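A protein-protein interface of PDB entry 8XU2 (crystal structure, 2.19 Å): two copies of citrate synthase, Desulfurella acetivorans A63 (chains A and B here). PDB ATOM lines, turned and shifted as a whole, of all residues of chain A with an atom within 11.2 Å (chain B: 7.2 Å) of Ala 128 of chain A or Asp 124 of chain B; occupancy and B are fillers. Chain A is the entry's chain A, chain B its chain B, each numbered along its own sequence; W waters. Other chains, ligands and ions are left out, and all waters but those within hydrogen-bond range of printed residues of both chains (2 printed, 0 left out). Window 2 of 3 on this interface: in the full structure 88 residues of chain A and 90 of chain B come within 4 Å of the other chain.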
ATOM      1  N   GLU A 120      -9.682   3.535  14.875  1.00  0.00           N
ATOM      2  CA  GLU A 120      -9.433   3.736  13.453  1.00  0.00           C
ATOM      3  C   GLU A 120      -7.950   3.895  13.149  1.00  0.00           C
ATOM      4  O   GLU A 120      -7.512   3.421  12.105  1.00  0.00           O
ATOM      5  CB  GLU A 120     -10.137   4.961  12.849  1.00  0.00           C
ATOM      6  CG  GLU A 120     -11.545   4.684  12.406  1.00  0.00           C
ATOM      7  CD  GLU A 120     -11.725   3.503  11.469  1.00  0.00           C
ATOM      8  OE1 GLU A 120     -11.060   3.470  10.435  1.00  0.00           O
ATOM      9  OE2 GLU A 120     -12.513   2.616  11.811  1.00  0.00           O
ATOM     10  N   TYR A 121      -7.208   4.595  14.011  1.00  0.00           N
ATOM     11  CA  TYR A 121      -5.781   4.829  13.763  1.00  0.00           C
ATOM     12  C   TYR A 121      -4.984   3.531  13.800  1.00  0.00           C
ATOM     13  O   TYR A 121      -3.867   3.479  13.281  1.00  0.00           O
ATOM     14  CB  TYR A 121      -5.201   5.846  14.752  1.00  0.00           C
ATOM     15  CG  TYR A 121      -5.087   5.370  16.189  1.00  0.00           C
ATOM     16  CD1 TYR A 121      -4.096   4.489  16.592  1.00  0.00           C
ATOM     17  CD2 TYR A 121      -5.976   5.823  17.150  1.00  0.00           C
ATOM     18  CE1 TYR A 121      -4.006   4.058  17.913  1.00  0.00           C
ATOM     19  CE2 TYR A 121      -5.907   5.407  18.466  1.00  0.00           C
ATOM     20  CZ  TYR A 121      -4.922   4.513  18.849  1.00  0.00           C
ATOM     21  OH  TYR A 121      -4.850   4.160  20.159  1.00  0.00           O
ATOM     22  N   VAL A 122      -5.534   2.467  14.400  1.00  0.00           N
ATOM     23  CA  VAL A 122      -4.868   1.170  14.330  1.00  0.00           C
ATOM     24  C   VAL A 122      -4.922   0.650  12.886  1.00  0.00           C
ATOM     25  O   VAL A 122      -3.922   0.152  12.352  1.00  0.00           O
ATOM     26  CB  VAL A 122      -5.460   0.160  15.333  1.00  0.00           C
ATOM     27  CG1 VAL A 122      -5.011  -1.270  15.034  1.00  0.00           C
ATOM     28  CG2 VAL A 122      -5.082   0.523  16.748  1.00  0.00           C
ATOM     29  N   LYS A 123      -6.072   0.773  12.258  1.00  0.00           N
ATOM     30  CA  LYS A 123      -6.234   0.397  10.857  1.00  0.00           C
ATOM     31  C   LYS A 123      -5.369   1.281   9.970  1.00  0.00           C
ATOM     32  O   LYS A 123      -4.753   0.771   9.056  1.00  0.00           O
ATOM     33  CB  LYS A 123      -7.701   0.517  10.429  1.00  0.00           C
ATOM     34  CG  LYS A 123      -8.640  -0.318  11.279  1.00  0.00           C
ATOM     35  CD  LYS A 123     -10.056  -0.209  10.849  1.00  0.00           C
ATOM     36  CE  LYS A 123     -10.994  -0.784  11.885  1.00  0.00           C
ATOM     37  NZ  LYS A 123     -12.395  -0.753  11.409  1.00  0.00           N
ATOM     38  N   ASP A 124      -5.318   2.593  10.252  1.00  0.00           N
ATOM     39  CA  ASP A 124      -4.483   3.516   9.494  1.00  0.00           C
ATOM     40  C   ASP A 124      -3.032   3.058   9.560  1.00  0.00           C
ATOM     41  O   ASP A 124      -2.314   3.139   8.572  1.00  0.00           O
ATOM     42  CB  ASP A 124      -4.548   4.957  10.037  1.00  0.00           C
ATOM     43  CG  ASP A 124      -5.902   5.648  10.017  1.00  0.00           C
ATOM     44  OD1 ASP A 124      -6.681   5.303   9.136  1.00  0.00           O
ATOM     45  OD2 ASP A 124      -6.151   6.557  10.905  1.00  0.00           O
ATOM     46  N   THR A 125      -2.577   2.694  10.758  1.00  0.00           N
ATOM     47  CA  THR A 125      -1.194   2.307  10.996  1.00  0.00           C
ATOM     48  C   THR A 125      -0.861   1.015  10.232  1.00  0.00           C
ATOM     49  O   THR A 125       0.204   0.920   9.629  1.00  0.00           O
ATOM     50  CB  THR A 125      -0.920   2.176  12.499  1.00  0.00           C
ATOM     51  OG1 THR A 125      -1.171   3.437  13.145  1.00  0.00           O
ATOM     52  CG2 THR A 125       0.483   1.707  12.802  1.00  0.00           C
ATOM     53  N   LEU A 126      -1.768   0.025  10.260  1.00  0.00           N
ATOM     54  CA  LEU A 126      -1.558  -1.251   9.583  1.00  0.00           C
ATOM     55  C   LEU A 126      -1.573  -1.084   8.059  1.00  0.00           C
ATOM     56  O   LEU A 126      -0.979  -1.888   7.348  1.00  0.00           O
ATOM     57  CB  LEU A 126      -2.661  -2.241  10.003  1.00  0.00           C
ATOM     58  CG  LEU A 126      -2.586  -2.742  11.450  1.00  0.00           C
ATOM     59  CD1 LEU A 126      -3.724  -3.672  11.805  1.00  0.00           C
ATOM     60  CD2 LEU A 126      -1.281  -3.451  11.706  1.00  0.00           C
ATOM     61  N   LYS A 127      -2.319  -0.090   7.554  1.00  0.00           N
ATOM     62  CA  LYS A 127      -2.306   0.207   6.138  1.00  0.00           C
ATOM     63  C   LYS A 127      -1.021   0.911   5.724  1.00  0.00           C
ATOM     64  O   LYS A 127      -0.606   0.767   4.589  1.00  0.00           O
ATOM     65  CB  LYS A 127      -3.437   1.140   5.716  1.00  0.00           C
ATOM     66  CG  LYS A 127      -4.825   0.538   5.763  1.00  0.00           C
ATOM     67  CD  LYS A 127      -5.797   1.637   5.506  1.00  0.00           C
ATOM     68  CE  LYS A 127      -7.243   1.239   5.556  1.00  0.00           C
ATOM     69  NZ  LYS A 127      -8.035   2.379   5.034  1.00  0.00           N
ATOM     70  N   ALA A 128      -0.428   1.711   6.611  1.00  0.00           N
ATOM     71  CA  ALA A 128       0.778   2.445   6.269  1.00  0.00           C
ATOM     72  C   ALA A 128       1.972   1.488   6.283  1.00  0.00           C
ATOM     73  O   ALA A 128       2.939   1.658   5.552  1.00  0.00           O
ATOM     74  CB  ALA A 128       0.945   3.595   7.227  1.00  0.00           C
ATOM     75  N   MET A 129       1.907   0.475   7.142  1.00  0.00           N
ATOM     76  CA  MET A 129       2.873  -0.614   7.115  1.00  0.00           C
ATOM     77  C   MET A 129       2.722  -1.369   5.798  1.00  0.00           C
ATOM     78  O   MET A 129       1.597  -1.693   5.392  1.00  0.00           O
ATOM     79  CB  MET A 129       2.653  -1.567   8.297  1.00  0.00           C
ATOM     80  CG  MET A 129       3.022  -0.950   9.636  1.00  0.00           C
ATOM     81  SD  MET A 129       2.592  -2.100  11.008  1.00  0.00           S
ATOM     82  CE  MET A 129       4.112  -3.022  11.157  1.00  0.00           C
ATOM     83  N   PRO A 130       3.826  -1.676   5.073  1.00  0.00           N
ATOM     84  CA  PRO A 130       3.711  -2.441   3.836  1.00  0.00           C
ATOM     85  C   PRO A 130       2.860  -3.701   4.021  1.00  0.00           C
ATOM     86  O   PRO A 130       3.005  -4.413   5.010  1.00  0.00           O
ATOM     87  CB  PRO A 130       5.170  -2.740   3.482  1.00  0.00           C
ATOM     88  CG  PRO A 130       5.924  -1.581   4.070  1.00  0.00           C
ATOM     89  CD  PRO A 130       5.205  -1.257   5.358  1.00  0.00           C
ATOM     90  N   ARG A 131       1.964  -3.947   3.054  1.00  0.00           N
ATOM     91  CA  ARG A 131       1.010  -5.040   3.135  1.00  0.00           C
ATOM     92  C   ARG A 131       1.732  -6.384   3.184  1.00  0.00           C
ATOM     93  O   ARG A 131       1.139  -7.378   3.614  1.00  0.00           O
ATOM     94  CB  ARG A 131       0.046  -4.971   1.934  1.00  0.00           C
ATOM     95  CG  ARG A 131      -1.116  -5.966   1.990  1.00  0.00           C
ATOM     96  CD  ARG A 131      -2.106  -5.723   3.112  1.00  0.00           C
ATOM     97  NE  ARG A 131      -2.457  -4.325   3.225  1.00  0.00           N
ATOM     98  CZ  ARG A 131      -3.617  -3.770   2.848  1.00  0.00           C
ATOM     99  NH1 ARG A 131      -4.645  -4.538   2.502  1.00  0.00           N
ATOM    100  NH2 ARG A 131      -3.738  -2.445   2.842  1.00  0.00           N
ATOM    101  N   ASP A 132       3.007  -6.421   2.718  1.00  0.00           N
ATOM    102  CA  ASP A 132       3.753  -7.667   2.690  1.00  0.00           C
ATOM    103  C   ASP A 132       4.425  -7.915   4.052  1.00  0.00           C
ATOM    104  O   ASP A 132       5.146  -8.879   4.209  1.00  0.00           O
ATOM    105  CB  ASP A 132       4.742  -7.708   1.526  1.00  0.00           C
ATOM    106  CG  ASP A 132       5.739  -6.560   1.502  1.00  0.00           C
ATOM    107  OD1 ASP A 132       5.656  -5.683   2.356  1.00  0.00           O
ATOM    108  OD2 ASP A 132       6.605  -6.548   0.614  1.00  0.00           O
ATOM    109  N   THR A 133       4.186  -7.047   5.038  1.00  0.00           N
ATOM    110  CA  THR A 133       4.641  -7.270   6.401  1.00  0.00           C
ATOM    111  C   THR A 133       4.014  -8.534   7.009  1.00  0.00           C
ATOM    112  O   THR A 133       2.812  -8.798   6.859  1.00  0.00           O
ATOM    113  CB  THR A 133       4.353  -6.025   7.244  1.00  0.00           C
ATOM    114  OG1 THR A 133       5.052  -4.902   6.692  1.00  0.00           O
ATOM    115  CG2 THR A 133       4.738  -6.214   8.695  1.00  0.00           C
ATOM    116  N   THR A 137       4.118  -9.187  12.864  1.00  0.00           N
ATOM    117  CA  THR A 137       4.649  -7.837  12.962  1.00  0.00           C
ATOM    118  C   THR A 137       3.508  -6.828  13.004  1.00  0.00           C
ATOM    119  O   THR A 137       3.525  -5.883  13.782  1.00  0.00           O
ATOM    120  CB  THR A 137       5.649  -7.566  11.835  1.00  0.00           C
ATOM    121  OG1 THR A 137       6.640  -8.580  11.885  1.00  0.00           O
ATOM    122  CG2 THR A 137       6.288  -6.200  11.959  1.00  0.00           C
ATOM    123  N   MET A 138       2.499  -7.040  12.166  1.00  0.00           N
ATOM    124  CA  MET A 138       1.331  -6.186  12.154  1.00  0.00           C
ATOM    125  C   MET A 138       0.602  -6.268  13.498  1.00  0.00           C
ATOM    126  O   MET A 138       0.116  -5.250  14.014  1.00  0.00           O
ATOM    127  CB  MET A 138       0.370  -6.613  11.049  1.00  0.00           C
ATOM    128  CG  MET A 138       0.774  -6.133   9.676  1.00  0.00           C
ATOM    129  SD  MET A 138      -0.509  -6.449   8.454  1.00  0.00           S
ATOM    130  CE  MET A 138       0.237  -5.643   7.027  1.00  0.00           C
ATOM    131  N   ALA A 141       2.411  -4.488  16.220  1.00  0.00           N
ATOM    132  CA  ALA A 141       2.378  -3.068  15.944  1.00  0.00           C
ATOM    133  C   ALA A 141       1.026  -2.483  16.331  1.00  0.00           C
ATOM    134  O   ALA A 141       0.944  -1.407  16.914  1.00  0.00           O
ATOM    135  CB  ALA A 141       2.683  -2.846  14.477  1.00  0.00           C
ATOM    136  N   GLY A 142      -0.047  -3.199  15.998  1.00  0.00           N
ATOM    137  CA  GLY A 142      -1.400  -2.808  16.381  1.00  0.00           C
ATOM    138  C   GLY A 142      -1.579  -2.654  17.894  1.00  0.00           C
ATOM    139  O   GLY A 142      -2.178  -1.686  18.353  1.00  0.00           O
ATOM    140  N   ALA A 145       0.535   0.437  19.060  1.00  0.00           N
ATOM    141  CA  ALA A 145      -0.052   1.727  18.717  1.00  0.00           C
ATOM    142  C   ALA A 145      -1.116   2.127  19.744  1.00  0.00           C
ATOM    143  O   ALA A 145      -1.259   3.320  20.043  1.00  0.00           O
ATOM    144  CB  ALA A 145      -0.642   1.663  17.333  1.00  0.00           C
ATOM    145  N   TYR A 187      -8.811  -8.280  11.628  1.00  0.00           N
ATOM    146  CA  TYR A 187      -8.540  -7.199  10.710  1.00  0.00           C
ATOM    147  C   TYR A 187      -7.342  -7.574   9.844  1.00  0.00           C
ATOM    148  O   TYR A 187      -7.381  -7.425   8.626  1.00  0.00           O
ATOM    149  CB  TYR A 187      -8.250  -5.871  11.421  1.00  0.00           C
ATOM    150  CG  TYR A 187      -8.193  -4.744  10.431  1.00  0.00           C
ATOM    151  CD1 TYR A 187      -9.371  -4.166   9.989  1.00  0.00           C
ATOM    152  CD2 TYR A 187      -6.993  -4.332   9.843  1.00  0.00           C
ATOM    153  CE1 TYR A 187      -9.368  -3.188   9.011  1.00  0.00           C
ATOM    154  CE2 TYR A 187      -6.983  -3.354   8.853  1.00  0.00           C
ATOM    155  CZ  TYR A 187      -8.178  -2.797   8.433  1.00  0.00           C
ATOM    156  OH  TYR A 187      -8.292  -1.806   7.481  1.00  0.00           O
ATOM    157  N   ILE A 188      -6.263  -8.010  10.490  1.00  0.00           N
ATOM    158  CA  ILE A 188      -5.040  -8.406   9.800  1.00  0.00           C
ATOM    159  C   ILE A 188      -5.335  -9.563   8.837  1.00  0.00           C
ATOM    160  O   ILE A 188      -4.834  -9.563   7.718  1.00  0.00           O
ATOM    161  CB  ILE A 188      -3.947  -8.757  10.829  1.00  0.00           C
ATOM    162  CG1 ILE A 188      -3.475  -7.505  11.561  1.00  0.00           C
ATOM    163  CG2 ILE A 188      -2.796  -9.528  10.208  1.00  0.00           C
ATOM    164  CD1 ILE A 188      -2.784  -7.793  12.866  1.00  0.00           C
ATOM    165  N   MET A 191      -7.353  -8.090   5.822  1.00  0.00           N
ATOM    166  CA  MET A 191      -6.594  -7.119   5.039  1.00  0.00           C
ATOM    167  C   MET A 191      -5.486  -7.793   4.229  1.00  0.00           C
ATOM    168  O   MET A 191      -5.194  -7.342   3.125  1.00  0.00           O
ATOM    169  CB  MET A 191      -5.997  -6.041   5.953  1.00  0.00           C
ATOM    170  CG  MET A 191      -4.511  -6.188   6.134  1.00  0.00           C
ATOM    171  SD  MET A 191      -3.902  -4.986   7.210  1.00  0.00           S
ATOM    172  CE  MET A 191      -4.026  -3.484   6.262  1.00  0.00           C
ATOM    173  N   LYS A 192      -4.886  -8.861   4.770  1.00  0.00           N
ATOM    174  CA  LYS A 192      -3.792  -9.566   4.111  1.00  0.00           C
ATOM    175  C   LYS A 192      -4.305 -10.673   3.194  1.00  0.00           C
ATOM    176  O   LYS A 192      -3.825 -10.786   2.077  1.00  0.00           O
ATOM    177  CB  LYS A 192      -2.804 -10.171   5.122  1.00  0.00           C
ATOM    178  CG  LYS A 192      -1.722  -9.202   5.595  1.00  0.00           C
ATOM    179  CD  LYS A 192      -0.625  -9.872   6.364  1.00  0.00           C
ATOM    180  CE  LYS A 192       0.349 -10.667   5.519  1.00  0.00           C
ATOM    181  NZ  LYS A 192       1.328  -9.792   4.831  1.00  0.00           N
ATOM    182  N   ASP A 196      -9.061  -7.832   1.542  1.00  0.00           N
ATOM    183  CA  ASP A 196      -9.248  -6.561   2.219  1.00  0.00           C
ATOM    184  C   ASP A 196     -10.717  -6.171   2.196  1.00  0.00           C
ATOM    185  O   ASP A 196     -11.044  -4.983   2.152  1.00  0.00           O
ATOM    186  CB  ASP A 196      -8.335  -5.478   1.628  1.00  0.00           C
ATOM    187  CG  ASP A 196      -8.020  -4.306   2.554  1.00  0.00           C
ATOM    188  OD1 ASP A 196      -8.319  -4.402   3.790  1.00  0.00           O
ATOM    189  OD2 ASP A 196      -7.487  -3.279   2.030  1.00  0.00           O
ATOM    190  N   PRO B 119      13.703   3.890   5.716  1.00  0.00           N
ATOM    191  CA  PRO B 119      12.609   3.554   4.803  1.00  0.00           C
ATOM    192  C   PRO B 119      11.462   4.551   4.886  1.00  0.00           C
ATOM    193  O   PRO B 119      11.092   4.957   5.982  1.00  0.00           O
ATOM    194  CB  PRO B 119      12.167   2.176   5.303  1.00  0.00           C
ATOM    195  CG  PRO B 119      13.419   1.577   5.892  1.00  0.00           C
ATOM    196  CD  PRO B 119      14.132   2.749   6.545  1.00  0.00           C
ATOM    197  N   GLU B 120      10.935   4.986   3.731  1.00  0.00           N
ATOM    198  CA  GLU B 120       9.829   5.935   3.703  1.00  0.00           C
ATOM    199  C   GLU B 120       8.601   5.376   4.436  1.00  0.00           C
ATOM    200  O   GLU B 120       7.892   6.154   5.035  1.00  0.00           O
ATOM    201  CB  GLU B 120       9.355   6.237   2.269  1.00  0.00           C
ATOM    202  CG  GLU B 120      10.078   7.369   1.612  1.00  0.00           C
ATOM    203  CD  GLU B 120      10.091   8.662   2.398  1.00  0.00           C
ATOM    204  OE1 GLU B 120       9.020   9.146   2.785  1.00  0.00           O
ATOM    205  OE2 GLU B 120      11.204   9.179   2.627  1.00  0.00           O
ATOM    206  N   TYR B 121       8.333   4.071   4.358  1.00  0.00           N
ATOM    207  CA  TYR B 121       7.168   3.489   5.026  1.00  0.00           C
ATOM    208  C   TYR B 121       7.285   3.591   6.548  1.00  0.00           C
ATOM    209  O   TYR B 121       6.273   3.492   7.255  1.00  0.00           O
ATOM    210  CB  TYR B 121       6.928   2.038   4.616  1.00  0.00           C
ATOM    211  CG  TYR B 121       7.964   1.046   5.085  1.00  0.00           C
ATOM    212  CD1 TYR B 121       8.000   0.596   6.404  1.00  0.00           C
ATOM    213  CD2 TYR B 121       8.885   0.520   4.202  1.00  0.00           C
ATOM    214  CE1 TYR B 121       8.949  -0.328   6.822  1.00  0.00           C
ATOM    215  CE2 TYR B 121       9.832  -0.423   4.598  1.00  0.00           C
ATOM    216  CZ  TYR B 121       9.864  -0.832   5.915  1.00  0.00           C
ATOM    217  OH  TYR B 121      10.783  -1.765   6.276  1.00  0.00           O
ATOM    218  N   VAL B 122       8.500   3.796   7.073  1.00  0.00           N
ATOM    219  CA  VAL B 122       8.624   4.052   8.509  1.00  0.00           C
ATOM    220  C   VAL B 122       8.007   5.416   8.839  1.00  0.00           C
ATOM    221  O   VAL B 122       7.271   5.564   9.818  1.00  0.00           O
ATOM    222  CB  VAL B 122      10.079   3.937   8.982  1.00  0.00           C
ATOM    223  CG1 VAL B 122      10.287   4.531  10.354  1.00  0.00           C
ATOM    224  CG2 VAL B 122      10.555   2.495   8.956  1.00  0.00           C
ATOM    225  N   LYS B 123       8.306   6.418   8.019  1.00  0.00           N
ATOM    226  CA  LYS B 123       7.697   7.736   8.160  1.00  0.00           C
ATOM    227  C   LYS B 123       6.192   7.664   7.960  1.00  0.00           C
ATOM    228  O   LYS B 123       5.467   8.286   8.696  1.00  0.00           O
ATOM    229  CB  LYS B 123       8.311   8.715   7.162  1.00  0.00           C
ATOM    230  CG  LYS B 123       9.810   8.835   7.296  1.00  0.00           C
ATOM    231  CD  LYS B 123      10.409   9.796   6.321  1.00  0.00           C
ATOM    232  CE  LYS B 123      11.912   9.630   6.260  1.00  0.00           C
ATOM    233  NZ  LYS B 123      12.514  10.666   5.396  1.00  0.00           N
ATOM    234  N   ASP B 124       5.728   6.901   6.972  1.00  0.00           N
ATOM    235  CA  ASP B 124       4.306   6.721   6.726  1.00  0.00           C
ATOM    236  C   ASP B 124       3.634   6.154   7.975  1.00  0.00           C
ATOM    237  O   ASP B 124       2.524   6.552   8.325  1.00  0.00           O
ATOM    238  CB  ASP B 124       4.022   5.771   5.554  1.00  0.00           C
ATOM    239  CG  ASP B 124       4.560   6.158   4.179  1.00  0.00           C
ATOM    240  OD1 ASP B 124       4.719   7.349   3.947  1.00  0.00           O
ATOM    241  OD2 ASP B 124       4.836   5.221   3.328  1.00  0.00           O
ATOM    242  N   THR B 125       4.261   5.146   8.585  1.00  0.00           N
ATOM    243  CA  THR B 125       3.712   4.464   9.755  1.00  0.00           C
ATOM    244  C   THR B 125       3.624   5.431  10.947  1.00  0.00           C
ATOM    245  O   THR B 125       2.612   5.448  11.650  1.00  0.00           O
ATOM    246  CB  THR B 125       4.529   3.213  10.107  1.00  0.00           C
ATOM    247  OG1 THR B 125       4.557   2.315   8.993  1.00  0.00           O
ATOM    248  CG2 THR B 125       3.968   2.504  11.327  1.00  0.00           C
ATOM    249  N   LEU B 126       4.672   6.238  11.164  1.00  0.00           N
ATOM    250  CA  LEU B 126       4.711   7.187  12.278  1.00  0.00           C
ATOM    251  C   LEU B 126       3.710   8.322  12.080  1.00  0.00           C
ATOM    252  O   LEU B 126       3.273   8.929  13.048  1.00  0.00           O
ATOM    253  CB  LEU B 126       6.122   7.768  12.421  1.00  0.00           C
ATOM    254  CG  LEU B 126       7.216   6.798  12.872  1.00  0.00           C
ATOM    255  CD1 LEU B 126       8.588   7.461  12.917  1.00  0.00           C
ATOM    256  CD2 LEU B 126       6.916   6.197  14.174  1.00  0.00           C
ATOM    257  N   LYS B 127       3.407   8.667  10.822  1.00  0.00           N
ATOM    258  CA  LYS B 127       2.386   9.659  10.542  1.00  0.00           C
ATOM    259  C   LYS B 127       0.989   9.093  10.753  1.00  0.00           C
ATOM    260  O   LYS B 127       0.086   9.849  11.064  1.00  0.00           O
ATOM    261  CB  LYS B 127       2.411  10.131   9.088  1.00  0.00           C
ATOM    262  CG  LYS B 127       3.607  10.987   8.711  1.00  0.00           C
ATOM    263  CD  LYS B 127       3.557  11.233   7.257  1.00  0.00           C
ATOM    264  CE  LYS B 127       4.675  12.090   6.744  1.00  0.00           C
ATOM    265  NZ  LYS B 127       4.421  12.414   5.320  1.00  0.00           N
ATOM    266  N   ALA B 128       0.786   7.794  10.525  1.00  0.00           N
ATOM    267  CA  ALA B 128      -0.529   7.195  10.687  1.00  0.00           C
ATOM    268  C   ALA B 128      -0.837   7.025  12.168  1.00  0.00           C
ATOM    269  O   ALA B 128      -1.989   7.129  12.596  1.00  0.00           O
ATOM    270  CB  ALA B 128      -0.587   5.880   9.949  1.00  0.00           C
ATOM    271  N   MET B 129       0.212   6.775  12.962  1.00  0.00           N
ATOM    272  CA  MET B 129       0.096   6.800  14.410  1.00  0.00           C
ATOM    273  C   MET B 129      -0.263   8.218  14.851  1.00  0.00           C
ATOM    274  O   MET B 129       0.338   9.194  14.383  1.00  0.00           O
ATOM    275  CB  MET B 129       1.412   6.380  15.064  1.00  0.00           C
ATOM    276  CG  MET B 129       1.730   4.892  14.867  1.00  0.00           C
ATOM    277  SD  MET B 129       3.371   4.440  15.457  1.00  0.00           S
ATOM    278  CE  MET B 129       2.932   3.991  17.134  1.00  0.00           C
ATOM    279  N   TYR B 187      13.915  11.811  13.369  1.00  0.00           N
ATOM    280  CA  TYR B 187      12.672  11.974  12.664  1.00  0.00           C
ATOM    281  C   TYR B 187      11.553  12.238  13.661  1.00  0.00           C
ATOM    282  O   TYR B 187      10.755  13.160  13.472  1.00  0.00           O
ATOM    283  CB  TYR B 187      12.304  10.753  11.812  1.00  0.00           C
ATOM    284  CG  TYR B 187      11.113  11.057  10.939  1.00  0.00           C
ATOM    285  CD1 TYR B 187      11.293  11.764   9.763  1.00  0.00           C
ATOM    286  CD2 TYR B 187       9.814  10.764  11.343  1.00  0.00           C
ATOM    287  CE1 TYR B 187      10.217  12.140   8.989  1.00  0.00           C
ATOM    288  CE2 TYR B 187       8.723  11.137  10.559  1.00  0.00           C
ATOM    289  CZ  TYR B 187       8.932  11.868   9.402  1.00  0.00           C
ATOM    290  OH  TYR B 187       7.963  12.278   8.506  1.00  0.00           O
HETATM  291  O   HOH W   1      -4.098   8.304  11.614  1.00  0.00           O
HETATM  292  O   HOH W   2       3.085   2.961   3.351  1.00  0.00           O
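Water W2 bridges the backbone carbonyl oxygen (O) of Ala 128 of chain A (2.6 Å) and the side-chain carboxylate (OD2) of Asp 124 of chain B (2.9 Å).
Water W1 lies within hydrogen-bond range of the backbone carbonyl oxygen of Ala 128 of chain B and the side-chain carboxylate of Asp 124 of chain A.
Ala 128 of chain A touches three residues of chain B.
Asp 124 of chain B touches just one residue of chain A: Ala 128.
No residue of chain A comes within 4 Å of Glu 120 of chain B.
Of chain A, only Thr 125, Ala 128 and Met 129 come within 4 Å of Thr 125 of chain B.
No residue of chain A comes within 4 Å of Leu 126 of chain B.
No residue of chain A comes within 4 Å of Lys 127 of chain B.
Printed residues of chain A within 4 Å of Ala 128 of chain B: Asp 124 (3.5 Å), Thr 125 (3.7 Å) and Ala 128 (3.9 Å).
Of the printed residues of chain A, Tyr 121 of chain B touches Pro 130 (3.5 Å).
Of the printed residues of chain B, Thr 125 of chain A touches Thr 125 (3.9 Å), Ala 128 (3.7 Å) and Met 129 (3.6 Å).
Printed residues of chain B within 4 Å of Asp 124 of chain A: Ala 128 (3.5 Å).
Leu 126 of chain A touches none of the printed residues of chain B.
Tyr 187 of chain A touches none of the printed residues of chain B.
The nearest printed residue of chain A that does not touch Asp 124 of chain B is Met 129 of chain A (5.9 Å).
The nearest printed residue of chain B that does not touch Met 129 of chain A is Tyr 121 of chain B (5.3 Å).
O of Tyr 121 of chain B sits at hydrogen-bond distance from OG1 of Thr 125 of chain B (2.7 Å).
The backbone carbonyl oxygen of Tyr 121 of chain A lies within hydrogen-bond range of the side-chain hydroxyl of Thr 125 of chain A (2.7 Å).
The backbone carbonyl oxygen (O) of Pro 130 of chain A sits at hydrogen-bond distance from the side-chain hydroxyl (OG1) of Thr 133 of chain A (2.7 Å).
Hydrophobic or aromatic side chains of chain A within 4 Å of the printed part of chain B: Ala 128, Met 129 and Pro 130.
Of the 12 printed residues of chain B, 5 touch a printed residue of chain A.
Hydrophobic or aromatic side chains of chain B within 4 Å of the printed part of chain A: Tyr 121, Ala 128 and Met 129.
Among the printed residues, no Asp or Glu carboxylate lies within 4 Å of a Lys or Arg side-chain nitrogen of the other chain.
Thr 125 of chain A touches its own counterpart, Thr 125 of chain B.
Thr 125 of chain A touches Ala 128 of chain B, and with the chains exchanged Ala 128 of chain A touches Thr 125 of chain B.
Thr 125 of chain A touches Met 129 of chain B, and with the chains exchanged Met 129 of chain A touches Thr 125 of chain B.
Ala 128 of chain B touches its own counterpart, Ala 128 of chain A.
11 positions are printed for both chains.
Of the 9 pairs that touch across the chains among the printed residues, 8 have their exchanged pair printed and touching as well.
Among the printed residues, merely in contact across the chains: Asp 124 of chain A with Ala 128 of chain B (3.5 Å), Thr 125 of chain A with Thr 125 of chain B (3.9 Å), Thr 125 of chain A with Ala 128 of chain B (3.7 Å), Thr 125 of chain A with Met 129 of chain B (3.6 Å), Ala 128 of chain A with Asp 124 of chain B (3.5 Å), Ala 128 of chain A with Thr 125 of chain B (3.8 Å), Ala 128 of chain A with Ala 128 of chain B (3.9 Å), Met 129 of chain A with Thr 125 of chain B (3.7 Å) and Pro 130 of chain A with Tyr 121 of chain B (3.5 Å).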
